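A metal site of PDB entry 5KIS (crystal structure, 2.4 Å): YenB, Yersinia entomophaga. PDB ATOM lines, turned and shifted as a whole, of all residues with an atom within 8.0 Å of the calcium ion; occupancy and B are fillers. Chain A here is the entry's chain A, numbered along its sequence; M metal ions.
The backbone carbonyl oxygen (O) of Asp 629 lies within hydrogen-bond range of the indole nitrogen (NE1) of Trp 710 (3.5 Å). The side-chain hydroxyl (OG1) of Thr 633 sits close to the backbone carbonyl oxygen (O) of Asn 649, 3.0 Å away. The backbone NH (N) of Asn 649 sits close to the side-chain carboxylate (OD1) of Asp 635, 2.7 Å away. OD2 of Asp 635 lies close to N of Ile 628 (2.8 Å). O of Ala 626 sits at hydrogen-bond distance from N of Asp 635 (3.0 Å). N of Gly 630 lies close to OD1 of Asp 627 (3.2 Å). N of Gly 632 is in hydrogen-bond range of OD2 of Asp 627, at 2.8 Å.
Of the 21 residues printed, 5 come within 4 Å of the calcium ion. Along chain A the residues within 4 Å of the calcium ion span positions 627 to 635. The nearest printed residue that does not touch the calcium ion is Asn 649 (4.2 Å).
The calcium ion is bound by the side-chain carboxylate (OD1) of Asp 629, the backbone carbonyl oxygen (O) of Thr 633, the side-chain hydroxyl (OG) of Ser 631, the side-chain carboxylate (OD2) of Asp 635, the side-chain carboxylate (OD1) of Asp 627, the side-chain carboxylate (OD1) of Asp 635 and the side-chain hydroxyl (OG1) of Thr 633.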
ATOM      1  N   SER A 354     -11.648  18.413  30.996  1.00  0.00           N
ATOM      2  CA  SER A 354     -11.874  17.859  29.670  1.00  0.00           C
ATOM      3  C   SER A 354     -12.370  16.428  29.749  1.00  0.00           C
ATOM      4  O   SER A 354     -13.441  16.117  29.221  1.00  0.00           O
ATOM      5  CB  SER A 354     -10.613  17.932  28.807  1.00  0.00           C
ATOM      6  OG  SER A 354      -9.979  19.182  28.982  1.00  0.00           O
ATOM      7  N   VAL A 355     -11.590  15.567  30.398  1.00  0.00           N
ATOM      8  CA  VAL A 355     -11.883  14.127  30.480  1.00  0.00           C
ATOM      9  C   VAL A 355     -11.440  13.538  31.842  1.00  0.00           C
ATOM     10  O   VAL A 355     -10.252  13.561  32.178  1.00  0.00           O
ATOM     11  CB  VAL A 355     -11.169  13.332  29.351  1.00  0.00           C
ATOM     12  CG1 VAL A 355     -11.407  11.834  29.487  1.00  0.00           C
ATOM     13  CG2 VAL A 355     -11.645  13.811  27.990  1.00  0.00           C
ATOM     14  N   ASP A 574     -17.941  20.305  15.743  1.00  0.00           N
ATOM     15  CA  ASP A 574     -18.295  19.660  17.015  1.00  0.00           C
ATOM     16  C   ASP A 574     -17.584  20.365  18.181  1.00  0.00           C
ATOM     17  O   ASP A 574     -16.477  20.019  18.576  1.00  0.00           O
ATOM     18  CB  ASP A 574     -17.961  18.165  16.990  1.00  0.00           C
ATOM     19  CG  ASP A 574     -18.585  17.401  18.156  1.00  0.00           C
ATOM     20  OD1 ASP A 574     -19.235  17.997  19.042  1.00  0.00           O
ATOM     21  OD2 ASP A 574     -18.416  16.171  18.185  1.00  0.00           O
ATOM     22  N   ALA A 626      -9.989  22.681  15.648  1.00  0.00           N
ATOM     23  CA  ALA A 626      -9.542  21.300  15.518  1.00  0.00           C
ATOM     24  C   ALA A 626      -9.319  20.674  16.887  1.00  0.00           C
ATOM     25  O   ALA A 626      -8.840  21.345  17.795  1.00  0.00           O
ATOM     26  CB  ALA A 626      -8.258  21.241  14.723  1.00  0.00           C
ATOM     27  N   ASP A 627      -9.677  19.403  17.031  1.00  0.00           N
ATOM     28  CA  ASP A 627      -9.420  18.668  18.265  1.00  0.00           C
ATOM     29  C   ASP A 627      -7.909  18.401  18.401  1.00  0.00           C
ATOM     30  O   ASP A 627      -7.399  17.431  17.835  1.00  0.00           O
ATOM     31  CB  ASP A 627     -10.237  17.374  18.280  1.00  0.00           C
ATOM     32  CG  ASP A 627     -10.297  16.699  19.658  1.00  0.00           C
ATOM     33  OD1 ASP A 627      -9.887  17.302  20.677  1.00  0.00           O
ATOM     34  OD2 ASP A 627     -10.773  15.544  19.735  1.00  0.00           O
ATOM     35  N   ILE A 628      -7.214  19.270  19.138  1.00  0.00           N
ATOM     36  CA  ILE A 628      -5.769  19.151  19.383  1.00  0.00           C
ATOM     37  C   ILE A 628      -5.428  18.052  20.386  1.00  0.00           C
ATOM     38  O   ILE A 628      -4.430  17.335  20.210  1.00  0.00           O
ATOM     39  CB  ILE A 628      -5.183  20.481  19.926  1.00  0.00           C
ATOM     40  CG1 ILE A 628      -5.420  21.654  18.952  1.00  0.00           C
ATOM     41  CG2 ILE A 628      -3.688  20.346  20.225  1.00  0.00           C
ATOM     42  CD1 ILE A 628      -4.827  21.482  17.566  1.00  0.00           C
ATOM     43  N   ASP A 629      -6.238  17.923  21.438  1.00  0.00           N
ATOM     44  CA  ASP A 629      -5.969  16.980  22.538  1.00  0.00           C
ATOM     45  C   ASP A 629      -6.769  15.660  22.448  1.00  0.00           C
ATOM     46  O   ASP A 629      -6.804  14.898  23.413  1.00  0.00           O
ATOM     47  CB  ASP A 629      -6.204  17.684  23.900  1.00  0.00           C
ATOM     48  CG  ASP A 629      -7.692  17.953  24.204  1.00  0.00           C
ATOM     49  OD1 ASP A 629      -8.499  18.058  23.260  1.00  0.00           O
ATOM     50  OD2 ASP A 629      -8.061  18.092  25.405  1.00  0.00           O
ATOM     51  N   GLY A 630      -7.418  15.399  21.317  1.00  0.00           N
ATOM     52  CA  GLY A 630      -8.193  14.169  21.136  1.00  0.00           C
ATOM     53  C   GLY A 630      -9.289  13.911  22.165  1.00  0.00           C
ATOM     54  O   GLY A 630      -9.686  12.765  22.376  1.00  0.00           O
ATOM     55  N   SER A 631      -9.801  14.967  22.791  1.00  0.00           N
ATOM     56  CA  SER A 631     -10.822  14.834  23.822  1.00  0.00           C
ATOM     57  C   SER A 631     -12.205  14.590  23.249  1.00  0.00           C
ATOM     58  O   SER A 631     -13.125  14.218  23.979  1.00  0.00           O
ATOM     59  CB  SER A 631     -10.866  16.092  24.691  1.00  0.00           C
ATOM     60  OG  SER A 631     -11.271  17.229  23.949  1.00  0.00           O
ATOM     61  N   GLY A 632     -12.364  14.787  21.945  1.00  0.00           N
ATOM     62  CA  GLY A 632     -13.668  14.798  21.311  1.00  0.00           C
ATOM     63  C   GLY A 632     -14.163  16.198  20.991  1.00  0.00           C
ATOM     64  O   GLY A 632     -15.049  16.328  20.153  1.00  0.00           O
ATOM     65  N   THR A 633     -13.596  17.229  21.626  1.00  0.00           N
ATOM     66  CA  THR A 633     -14.061  18.608  21.461  1.00  0.00           C
ATOM     67  C   THR A 633     -13.131  19.428  20.611  1.00  0.00           C
ATOM     68  O   THR A 633     -11.918  19.426  20.854  1.00  0.00           O
ATOM     69  CB  THR A 633     -14.118  19.335  22.814  1.00  0.00           C
ATOM     70  OG1 THR A 633     -12.834  19.258  23.462  1.00  0.00           O
ATOM     71  CG2 THR A 633     -15.201  18.752  23.696  1.00  0.00           C
ATOM     72  N   ASN A 634     -13.682  20.175  19.652  1.00  0.00           N
ATOM     73  CA  ASN A 634     -12.861  21.055  18.812  1.00  0.00           C
ATOM     74  C   ASN A 634     -12.337  22.199  19.641  1.00  0.00           C
ATOM     75  O   ASN A 634     -13.073  22.832  20.401  1.00  0.00           O
ATOM     76  CB  ASN A 634     -13.637  21.596  17.618  1.00  0.00           C
ATOM     77  CG  ASN A 634     -13.635  20.647  16.437  1.00  0.00           C
ATOM     78  OD1 ASN A 634     -12.726  20.668  15.615  1.00  0.00           O
ATOM     79  ND2 ASN A 634     -14.658  19.814  16.337  1.00  0.00           N
ATOM     80  N   ASP A 635     -11.046  22.461  19.497  1.00  0.00           N
ATOM     81  CA  ASP A 635     -10.347  23.523  20.218  1.00  0.00           C
ATOM     82  C   ASP A 635     -10.143  24.729  19.315  1.00  0.00           C
ATOM     83  O   ASP A 635     -10.301  24.626  18.107  1.00  0.00           O
ATOM     84  CB  ASP A 635      -9.015  22.969  20.710  1.00  0.00           C
ATOM     85  CG  ASP A 635      -9.188  21.672  21.505  1.00  0.00           C
ATOM     86  OD1 ASP A 635      -9.855  21.739  22.562  1.00  0.00           O
ATOM     87  OD2 ASP A 635      -8.698  20.596  21.099  1.00  0.00           O
ATOM     88  N   ILE A 636      -9.809  25.877  19.896  1.00  0.00           N
ATOM     89  CA  ILE A 636      -9.566  27.096  19.121  1.00  0.00           C
ATOM     90  C   ILE A 636      -8.077  27.334  19.003  1.00  0.00           C
ATOM     91  O   ILE A 636      -7.391  27.367  20.019  1.00  0.00           O
ATOM     92  CB  ILE A 636     -10.246  28.325  19.762  1.00  0.00           C
ATOM     93  CG1 ILE A 636     -11.765  28.241  19.576  1.00  0.00           C
ATOM     94  CG2 ILE A 636      -9.698  29.618  19.151  1.00  0.00           C
ATOM     95  CD1 ILE A 636     -12.556  29.317  20.290  1.00  0.00           C
ATOM     96  N   TYR A 647      -6.714  27.542  22.676  1.00  0.00           N
ATOM     97  CA  TYR A 647      -7.700  27.504  23.741  1.00  0.00           C
ATOM     98  C   TYR A 647      -8.302  26.103  23.744  1.00  0.00           C
ATOM     99  O   TYR A 647      -9.064  25.756  22.846  1.00  0.00           O
ATOM    100  CB  TYR A 647      -8.804  28.550  23.517  1.00  0.00           C
ATOM    101  CG  TYR A 647      -8.347  29.997  23.438  1.00  0.00           C
ATOM    102  CD1 TYR A 647      -7.744  30.497  22.282  1.00  0.00           C
ATOM    103  CD2 TYR A 647      -8.540  30.867  24.505  1.00  0.00           C
ATOM    104  CE1 TYR A 647      -7.329  31.824  22.195  1.00  0.00           C
ATOM    105  CE2 TYR A 647      -8.138  32.199  24.435  1.00  0.00           C
ATOM    106  CZ  TYR A 647      -7.538  32.668  23.277  1.00  0.00           C
ATOM    107  OH  TYR A 647      -7.130  33.971  23.215  1.00  0.00           O
ATOM    108  N   LEU A 648      -7.947  25.300  24.738  1.00  0.00           N
ATOM    109  CA  LEU A 648      -8.511  23.946  24.840  1.00  0.00           C
ATOM    110  C   LEU A 648      -9.966  23.993  25.278  1.00  0.00           C
ATOM    111  O   LEU A 648     -10.316  24.678  26.252  1.00  0.00           O
ATOM    112  CB  LEU A 648      -7.687  23.088  25.807  1.00  0.00           C
ATOM    113  CG  LEU A 648      -6.397  22.541  25.197  1.00  0.00           C
ATOM    114  CD1 LEU A 648      -5.380  22.262  26.290  1.00  0.00           C
ATOM    115  CD2 LEU A 648      -6.688  21.269  24.414  1.00  0.00           C
ATOM    116  N   ASN A 649     -10.811  23.272  24.554  1.00  0.00           N
ATOM    117  CA  ASN A 649     -12.225  23.188  24.854  1.00  0.00           C
ATOM    118  C   ASN A 649     -12.435  22.149  25.944  1.00  0.00           C
ATOM    119  O   ASN A 649     -12.100  20.972  25.767  1.00  0.00           O
ATOM    120  CB  ASN A 649     -12.979  22.768  23.589  1.00  0.00           C
ATOM    121  CG  ASN A 649     -14.473  22.714  23.786  1.00  0.00           C
ATOM    122  OD1 ASN A 649     -14.970  22.574  24.910  1.00  0.00           O
ATOM    123  ND2 ASN A 649     -15.212  22.793  22.681  1.00  0.00           N
ATOM    124  N   GLU A 650     -13.002  22.602  27.076  1.00  0.00           N
ATOM    125  CA  GLU A 650     -13.238  21.764  28.258  1.00  0.00           C
ATOM    126  C   GLU A 650     -14.622  21.127  28.241  1.00  0.00           C
ATOM    127  O   GLU A 650     -15.589  21.712  28.727  1.00  0.00           O
ATOM    128  CB  GLU A 650     -13.082  22.605  29.523  1.00  0.00           C
ATOM    129  CG  GLU A 650     -11.693  23.163  29.747  1.00  0.00           C
ATOM    130  CD  GLU A 650     -11.523  23.815  31.102  1.00  0.00           C
ATOM    131  OE1 GLU A 650     -12.538  23.996  31.836  1.00  0.00           O
ATOM    132  OE2 GLU A 650     -10.364  24.143  31.442  1.00  0.00           O
ATOM    133  N   SER A 651     -14.708  19.922  27.662  1.00  0.00           N
ATOM    134  CA  SER A 651     -15.959  19.158  27.624  1.00  0.00           C
ATOM    135  C   SER A 651     -17.170  20.022  27.210  1.00  0.00           C
ATOM    136  O   SER A 651     -18.256  19.894  27.760  1.00  0.00           O
ATOM    137  CB  SER A 651     -16.199  18.496  28.991  1.00  0.00           C
ATOM    138  OG  SER A 651     -17.148  17.441  28.917  1.00  0.00           O
ATOM    139  N   GLY A 652     -16.938  20.910  26.244  1.00  0.00           N
ATOM    140  CA  GLY A 652     -17.971  21.793  25.707  1.00  0.00           C
ATOM    141  C   GLY A 652     -18.562  22.826  26.640  1.00  0.00           C
ATOM    142  O   GLY A 652     -19.639  23.371  26.368  1.00  0.00           O
ATOM    143  N   TRP A 710      -6.253   9.785  26.373  1.00  0.00           N
ATOM    144  CA  TRP A 710      -7.434   9.158  27.042  1.00  0.00           C
ATOM    145  C   TRP A 710      -7.668   7.660  26.762  1.00  0.00           C
ATOM    146  O   TRP A 710      -8.736   7.135  27.038  1.00  0.00           O
ATOM    147  CB  TRP A 710      -8.715   9.958  26.799  1.00  0.00           C
ATOM    148  CG  TRP A 710      -8.489  11.411  26.870  1.00  0.00           C
ATOM    149  CD1 TRP A 710      -8.564  12.278  25.841  1.00  0.00           C
ATOM    150  CD2 TRP A 710      -8.105  12.170  28.013  1.00  0.00           C
ATOM    151  NE1 TRP A 710      -8.280  13.554  26.267  1.00  0.00           N
ATOM    152  CE2 TRP A 710      -7.986  13.520  27.603  1.00  0.00           C
ATOM    153  CE3 TRP A 710      -7.863  11.854  29.349  1.00  0.00           C
ATOM    154  CZ2 TRP A 710      -7.636  14.543  28.467  1.00  0.00           C
ATOM    155  CZ3 TRP A 710      -7.510  12.874  30.204  1.00  0.00           C
ATOM    156  CH2 TRP A 710      -7.408  14.210  29.763  1.00  0.00           C
HETATM  157 CA    CA M   1     -10.268  19.102  22.537  1.00  0.00          CA
